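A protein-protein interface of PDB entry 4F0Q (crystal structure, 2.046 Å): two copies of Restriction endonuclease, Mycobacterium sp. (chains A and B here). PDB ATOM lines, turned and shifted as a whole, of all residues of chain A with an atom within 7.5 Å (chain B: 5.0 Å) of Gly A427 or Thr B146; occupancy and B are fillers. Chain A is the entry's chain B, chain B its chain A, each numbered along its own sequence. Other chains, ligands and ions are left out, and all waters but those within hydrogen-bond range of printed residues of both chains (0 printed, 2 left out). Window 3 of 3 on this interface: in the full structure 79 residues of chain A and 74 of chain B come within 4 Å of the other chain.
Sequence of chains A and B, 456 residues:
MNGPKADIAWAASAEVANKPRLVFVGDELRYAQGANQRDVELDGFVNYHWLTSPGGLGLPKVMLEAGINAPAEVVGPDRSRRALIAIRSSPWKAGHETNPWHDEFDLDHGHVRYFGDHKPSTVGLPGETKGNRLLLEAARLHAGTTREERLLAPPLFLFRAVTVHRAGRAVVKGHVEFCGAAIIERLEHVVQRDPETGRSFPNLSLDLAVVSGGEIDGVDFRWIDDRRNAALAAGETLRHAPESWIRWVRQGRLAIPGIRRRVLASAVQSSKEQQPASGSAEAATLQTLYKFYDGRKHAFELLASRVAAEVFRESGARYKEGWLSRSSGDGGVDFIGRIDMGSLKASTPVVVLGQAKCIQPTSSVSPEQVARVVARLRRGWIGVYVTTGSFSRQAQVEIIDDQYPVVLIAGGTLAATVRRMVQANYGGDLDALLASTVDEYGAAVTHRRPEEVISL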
ATOM      1  N   VAL A 191      -8.636 -25.037   1.068  1.00  0.00           N
ATOM      2  CA  VAL A 191      -7.736 -23.901   1.222  1.00  0.00           C
ATOM      3  C   VAL A 191      -7.073 -23.592  -0.114  1.00  0.00           C
ATOM      4  O   VAL A 191      -6.427 -24.450  -0.715  1.00  0.00           O
ATOM      5  CB  VAL A 191      -6.666 -24.144   2.299  1.00  0.00           C
ATOM      6  CG1 VAL A 191      -5.643 -23.017   2.290  1.00  0.00           C
ATOM      7  CG2 VAL A 191      -7.315 -24.263   3.669  1.00  0.00           C
ATOM      8  N   ARG A 193      -4.978 -20.655  -2.868  1.00  0.00           N
ATOM      9  CA  ARG A 193      -3.994 -19.584  -2.943  1.00  0.00           C
ATOM     10  C   ARG A 193      -4.270 -18.721  -4.170  1.00  0.00           C
ATOM     11  O   ARG A 193      -4.627 -19.238  -5.233  1.00  0.00           O
ATOM     12  CB  ARG A 193      -2.579 -20.162  -3.012  1.00  0.00           C
ATOM     13  CG  ARG A 193      -1.482 -19.111  -2.946  1.00  0.00           C
ATOM     14  CD  ARG A 193      -0.103 -19.728  -3.075  1.00  0.00           C
ATOM     15  NE  ARG A 193       0.956 -18.734  -2.924  1.00  0.00           N
ATOM     16  CZ  ARG A 193       1.455 -18.013  -3.924  1.00  0.00           C
ATOM     17  NH1 ARG A 193       0.988 -18.171  -5.155  1.00  0.00           N
ATOM     18  NH2 ARG A 193       2.418 -17.132  -3.692  1.00  0.00           N
ATOM     19  N   GLY A 198      -0.677 -13.575  -3.948  1.00  0.00           N
ATOM     20  CA  GLY A 198       0.103 -14.488  -3.130  1.00  0.00           C
ATOM     21  C   GLY A 198      -0.503 -14.764  -1.768  1.00  0.00           C
ATOM     22  O   GLY A 198       0.174 -15.256  -0.867  1.00  0.00           O
ATOM     23  N   SER A 200      -3.253 -16.664   0.757  1.00  0.00           N
ATOM     24  CA  SER A 200      -4.005 -17.905   0.884  1.00  0.00           C
ATOM     25  C   SER A 200      -5.263 -17.681   1.715  1.00  0.00           C
ATOM     26  O   SER A 200      -5.291 -16.818   2.593  1.00  0.00           O
ATOM     27  CB  SER A 200      -3.135 -18.996   1.509  1.00  0.00           C
ATOM     28  OG  SER A 200      -1.965 -19.214   0.739  1.00  0.00           O
ATOM     29  N   MET A 421      -0.951 -28.596  -6.990  1.00  0.00           N
ATOM     30  CA  MET A 421      -0.145 -29.115  -5.888  1.00  0.00           C
ATOM     31  C   MET A 421       0.858 -28.074  -5.410  1.00  0.00           C
ATOM     32  O   MET A 421       0.990 -27.816  -4.211  1.00  0.00           O
ATOM     33  CB  MET A 421       0.605 -30.376  -6.324  1.00  0.00           C
ATOM     34  CG  MET A 421      -0.289 -31.558  -6.660  1.00  0.00           C
ATOM     35  SD  MET A 421       0.593 -32.863  -7.539  1.00  0.00           S
ATOM     36  CE  MET A 421       1.822 -33.330  -6.324  1.00  0.00           C
ATOM     37  N   VAL A 422       1.565 -27.482  -6.364  1.00  0.00           N
ATOM     38  CA  VAL A 422       2.557 -26.457  -6.080  1.00  0.00           C
ATOM     39  C   VAL A 422       1.924 -25.242  -5.405  1.00  0.00           C
ATOM     40  O   VAL A 422       2.437 -24.741  -4.402  1.00  0.00           O
ATOM     41  CB  VAL A 422       3.292 -26.032  -7.367  1.00  0.00           C
ATOM     42  CG1 VAL A 422       3.963 -24.693  -7.187  1.00  0.00           C
ATOM     43  CG2 VAL A 422       4.304 -27.091  -7.766  1.00  0.00           C
ATOM     44  N   GLN A 423       0.801 -24.779  -5.947  1.00  0.00           N
ATOM     45  CA  GLN A 423       0.103 -23.634  -5.371  1.00  0.00           C
ATOM     46  C   GLN A 423      -0.452 -23.928  -3.976  1.00  0.00           C
ATOM     47  O   GLN A 423      -0.572 -23.027  -3.147  1.00  0.00           O
ATOM     48  CB  GLN A 423      -1.020 -23.163  -6.299  1.00  0.00           C
ATOM     49  CG  GLN A 423      -0.534 -22.455  -7.554  1.00  0.00           C
ATOM     50  CD  GLN A 423      -0.043 -21.044  -7.282  1.00  0.00           C
ATOM     51  OE1 GLN A 423      -0.467 -20.401  -6.324  1.00  0.00           O
ATOM     52  NE2 GLN A 423       0.857 -20.558  -8.129  1.00  0.00           N
ATOM     53  N   ALA A 424      -0.778 -25.192  -3.717  1.00  0.00           N
ATOM     54  CA  ALA A 424      -1.416 -25.568  -2.457  1.00  0.00           C
ATOM     55  C   ALA A 424      -0.445 -26.068  -1.390  1.00  0.00           C
ATOM     56  O   ALA A 424      -0.842 -26.287  -0.246  1.00  0.00           O
ATOM     57  CB  ALA A 424      -2.501 -26.607  -2.703  1.00  0.00           C
ATOM     58  N   ASN A 425       0.821 -26.254  -1.754  1.00  0.00           N
ATOM     59  CA  ASN A 425       1.789 -26.805  -0.807  1.00  0.00           C
ATOM     60  C   ASN A 425       3.126 -26.068  -0.734  1.00  0.00           C
ATOM     61  O   ASN A 425       3.755 -26.020   0.325  1.00  0.00           O
ATOM     62  CB  ASN A 425       2.028 -28.292  -1.086  1.00  0.00           C
ATOM     63  CG  ASN A 425       0.769 -29.120  -0.932  1.00  0.00           C
ATOM     64  OD1 ASN A 425       0.355 -29.438   0.183  1.00  0.00           O
ATOM     65  ND2 ASN A 425       0.154 -29.476  -2.053  1.00  0.00           N
ATOM     66  N   TYR A 426       3.558 -25.494  -1.851  1.00  0.00           N
ATOM     67  CA  TYR A 426       4.870 -24.858  -1.906  1.00  0.00           C
ATOM     68  C   TYR A 426       4.803 -23.366  -2.219  1.00  0.00           C
ATOM     69  O   TYR A 426       5.743 -22.801  -2.775  1.00  0.00           O
ATOM     70  CB  TYR A 426       5.773 -25.576  -2.912  1.00  0.00           C
ATOM     71  CG  TYR A 426       5.971 -27.044  -2.605  1.00  0.00           C
ATOM     72  CD1 TYR A 426       6.836 -27.451  -1.597  1.00  0.00           C
ATOM     73  CD2 TYR A 426       5.294 -28.022  -3.322  1.00  0.00           C
ATOM     74  CE1 TYR A 426       7.021 -28.792  -1.311  1.00  0.00           C
ATOM     75  CE2 TYR A 426       5.473 -29.366  -3.044  1.00  0.00           C
ATOM     76  CZ  TYR A 426       6.337 -29.745  -2.038  1.00  0.00           C
ATOM     77  OH  TYR A 426       6.519 -31.081  -1.757  1.00  0.00           O
ATOM     78  N   GLY A 427       3.692 -22.734  -1.856  1.00  0.00           N
ATOM     79  CA  GLY A 427       3.526 -21.303  -2.034  1.00  0.00           C
ATOM     80  C   GLY A 427       3.659 -20.836  -3.472  1.00  0.00           C
ATOM     81  O   GLY A 427       4.061 -19.703  -3.729  1.00  0.00           O
ATOM     82  N   GLY A 428       3.322 -21.713  -4.411  1.00  0.00           N
ATOM     83  CA  GLY A 428       3.386 -21.375  -5.820  1.00  0.00           C
ATOM     84  C   GLY A 428       4.778 -21.511  -6.401  1.00  0.00           C
ATOM     85  O   GLY A 428       5.044 -21.038  -7.507  1.00  0.00           O
ATOM     86  N   ASP A 429       5.668 -22.165  -5.661  1.00  0.00           N
ATOM     87  CA  ASP A 429       7.040 -22.371  -6.117  1.00  0.00           C
ATOM     88  C   ASP A 429       7.230 -23.773  -6.692  1.00  0.00           C
ATOM     89  O   ASP A 429       7.323 -24.753  -5.953  1.00  0.00           O
ATOM     90  CB  ASP A 429       8.035 -22.119  -4.982  1.00  0.00           C
ATOM     91  CG  ASP A 429       9.472 -22.099  -5.459  1.00  0.00           C
ATOM     92  OD1 ASP A 429       9.696 -21.850  -6.664  1.00  0.00           O
ATOM     93  OD2 ASP A 429      10.380 -22.325  -4.632  1.00  0.00           O
ATOM     94  N   LEU A 430       7.283 -23.853  -8.018  1.00  0.00           N
ATOM     95  CA  LEU A 430       7.417 -25.120  -8.728  1.00  0.00           C
ATOM     96  C   LEU A 430       8.739 -25.810  -8.401  1.00  0.00           C
ATOM     97  O   LEU A 430       8.805 -27.039  -8.259  1.00  0.00           O
ATOM     98  CB  LEU A 430       7.314 -24.871 -10.234  1.00  0.00           C
ATOM     99  CG  LEU A 430       7.345 -26.069 -11.181  1.00  0.00           C
ATOM    100  CD1 LEU A 430       6.136 -26.957 -10.959  1.00  0.00           C
ATOM    101  CD2 LEU A 430       7.404 -25.597 -12.625  1.00  0.00           C
ATOM    102  N   ALA A 432      10.436 -25.908  -5.729  1.00  0.00           N
ATOM    103  CA  ALA A 432      10.430 -26.617  -4.457  1.00  0.00           C
ATOM    104  C   ALA A 432      10.022 -28.069  -4.680  1.00  0.00           C
ATOM    105  O   ALA A 432      10.675 -28.994  -4.190  1.00  0.00           O
ATOM    106  CB  ALA A 432       9.489 -25.941  -3.477  1.00  0.00           C
ATOM    107  N   GLY B 144      -2.442 -25.679   4.998  1.00  0.00           N
ATOM    108  CA  GLY B 144      -1.635 -24.501   4.737  1.00  0.00           C
ATOM    109  C   GLY B 144      -0.869 -24.607   3.433  1.00  0.00           C
ATOM    110  O   GLY B 144      -0.302 -25.653   3.119  1.00  0.00           O
ATOM    111  N   THR B 145      -0.849 -23.516   2.675  1.00  0.00           N
ATOM    112  CA  THR B 145      -0.245 -23.518   1.346  1.00  0.00           C
ATOM    113  C   THR B 145       1.275 -23.411   1.382  1.00  0.00           C
ATOM    114  O   THR B 145       1.935 -23.568   0.357  1.00  0.00           O
ATOM    115  CB  THR B 145      -0.807 -22.385   0.470  1.00  0.00           C
ATOM    116  OG1 THR B 145      -0.514 -21.120   1.076  1.00  0.00           O
ATOM    117  CG2 THR B 145      -2.313 -22.533   0.317  1.00  0.00           C
ATOM    118  N   THR B 146       1.827 -23.129   2.558  1.00  0.00           N
ATOM    119  CA  THR B 146       3.276 -23.056   2.720  1.00  0.00           C
ATOM    120  C   THR B 146       3.723 -23.823   3.957  1.00  0.00           C
ATOM    121  O   THR B 146       2.910 -24.158   4.819  1.00  0.00           O
ATOM    122  CB  THR B 146       3.768 -21.600   2.848  1.00  0.00           C
ATOM    123  OG1 THR B 146       3.172 -20.990   3.998  1.00  0.00           O
ATOM    124  CG2 THR B 146       3.410 -20.797   1.608  1.00  0.00           C
ATOM    125  N   ARG B 147       5.020 -24.097   4.038  1.00  0.00           N
ATOM    126  CA  ARG B 147       5.594 -24.745   5.209  1.00  0.00           C
ATOM    127  C   ARG B 147       5.443 -23.840   6.426  1.00  0.00           C
ATOM    128  O   ARG B 147       5.259 -24.312   7.548  1.00  0.00           O
ATOM    129  CB  ARG B 147       7.072 -25.066   4.971  1.00  0.00           C
ATOM    130  CG  ARG B 147       7.747 -25.765   6.137  1.00  0.00           C
ATOM    131  CD  ARG B 147       9.208 -26.062   5.851  1.00  0.00           C
ATOM    132  NE  ARG B 147       9.817 -26.848   6.920  1.00  0.00           N
ATOM    133  CZ  ARG B 147      10.365 -26.326   8.013  1.00  0.00           C
ATOM    134  NH1 ARG B 147      10.384 -25.011   8.186  1.00  0.00           N
ATOM    135  NH2 ARG B 147      10.895 -27.119   8.934  1.00  0.00           N
ATOM    136  N   GLU B 148       5.511 -22.534   6.187  1.00  0.00           N
ATOM    137  CA  GLU B 148       5.410 -21.545   7.250  1.00  0.00           C
ATOM    138  C   GLU B 148       4.030 -21.568   7.904  1.00  0.00           C
ATOM    139  O   GLU B 148       3.902 -21.364   9.112  1.00  0.00           O
ATOM    140  CB  GLU B 148       5.706 -20.149   6.701  1.00  0.00           C
ATOM    141  CG  GLU B 148       6.078 -19.135   7.764  1.00  0.00           C
ATOM    142  CD  GLU B 148       7.428 -19.422   8.390  1.00  0.00           C
ATOM    143  OE1 GLU B 148       8.326 -19.912   7.672  1.00  0.00           O
ATOM    144  OE2 GLU B 148       7.592 -19.163   9.601  1.00  0.00           O
ATOM    145  N   GLU B 149       3.001 -21.815   7.101  1.00  0.00           N
ATOM    146  CA  GLU B 149       1.639 -21.897   7.618  1.00  0.00           C
ATOM    147  C   GLU B 149       1.411 -23.209   8.359  1.00  0.00           C
ATOM    148  O   GLU B 149       0.723 -23.244   9.379  1.00  0.00           O
ATOM    149  CB  GLU B 149       0.617 -21.742   6.490  1.00  0.00           C
ATOM    150  CG  GLU B 149       0.583 -20.355   5.870  1.00  0.00           C
ATOM    151  CD  GLU B 149      -0.507 -20.207   4.827  1.00  0.00           C
ATOM    152  OE1 GLU B 149      -1.191 -21.210   4.529  1.00  0.00           O
ATOM    153  OE2 GLU B 149      -0.682 -19.086   4.306  1.00  0.00           O
ATOM    154  N   ARG B 150       1.995 -24.286   7.842  1.00  0.00           N
ATOM    155  CA  ARG B 150       1.836 -25.607   8.441  1.00  0.00           C
ATOM    156  C   ARG B 150       2.586 -25.728   9.764  1.00  0.00           C
ATOM    157  O   ARG B 150       2.273 -26.589  10.587  1.00  0.00           O
ATOM    158  CB  ARG B 150       2.282 -26.698   7.465  1.00  0.00           C
ATOM    159  CG  ARG B 150       1.411 -26.796   6.222  1.00  0.00           C
ATOM    160  CD  ARG B 150       1.788 -27.988   5.360  1.00  0.00           C
ATOM    161  NE  ARG B 150       3.091 -27.827   4.723  1.00  0.00           N
ATOM    162  CZ  ARG B 150       3.280 -27.230   3.550  1.00  0.00           C
ATOM    163  NH1 ARG B 150       2.248 -26.730   2.884  1.00  0.00           N
ATOM    164  NH2 ARG B 150       4.500 -27.130   3.044  1.00  0.00           N
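OG1 of Thr B145 sits at hydrogen-bond distance from OG of Ser A200 (2.4 Å).
N of Tyr A426 lies within hydrogen-bond range of O of Thr B145.
O of Thr B145 is in hydrogen-bond range of N of Gly A427, at 2.9 Å.
The backbone carbonyl oxygen (O) of Asn A425 lies within hydrogen-bond range of the guanidinium group (NH2) of Arg B150 (3.0 Å).
The backbone carbonyl oxygen of Gly B144 lies close to the backbone carbonyl oxygen of Ala A424.
The backbone carbonyl oxygen (O) of Asn A425 sits close to the backbone carbonyl oxygen (O) of Thr B145 (3.1 Å).
The backbone NH (N) of Glu B149 sits at hydrogen-bond distance from the side-chain hydroxyl (OG1) of Thr B146, 3.2 Å away.
The guanidinium group (NH1) of Arg B150 lies within hydrogen-bond range of the backbone carbonyl oxygen (O) of Thr B146 (3.3 Å).
The guanidinium group of Arg A193 sits at hydrogen-bond distance from the side-chain amide oxygen of Gln A423 (2.9 Å).
The guanidinium group (NH2) of Arg A193 sits at hydrogen-bond distance from the backbone carbonyl oxygen (O) of Gly A427 (3.1 Å).
O of Met A421 sits at hydrogen-bond distance from ND2 of Asn A425 (2.8 Å).
The backbone carbonyl oxygen of Val A422 is in hydrogen-bond range of the backbone NH of Gly A427, at 3.5 Å.
Among the printed residues, pairs that only touch across the chains: Ala A424 with Thr B145, Gly A427 with Thr B146, Gln A423 with Thr B145, Ser A200 with Glu B149, Asn A425 with Thr B146 and Val A191 with Thr B145.
Of the printed residues of chain B, Gly A427 touches Thr B145 (2.9 Å) and Thr B146 (3.7 Å).
Of the printed residues of chain A, Thr B146 touches Asn A425 and Gly A427.
Printed residues of chain B within 4 Å of Ser A200: Thr B145 (2.4 Å) and Glu B149 (3.7 Å).
Printed residues of chain B within 4 Å of Val A191: Thr B145 (3.9 Å).
Of the printed residues of chain B, Tyr A426 touches Thr B145 (3.3 Å).
Of the printed residues of chain A, Glu B149 touches Ser A200.
Of the printed residues of chain B, Asn A425 touches Thr B145, Thr B146 and Arg B150.
The nearest printed residue of chain B that does not touch Tyr A426 is Thr B146 (4.8 Å).
Of the 15 printed residues of chain A, 7 touch a printed residue of chain B.
Printed residues of chain A that touch a printed residue of chain B: Val A191, Ser A200, Gln A423, Ala A424, Asn A425, Tyr A426 and Gly A427.
Hydrophobic or aromatic side chains of chain A within 4 Å of the printed part of chain B: Val A191.
No position is printed for both chains.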
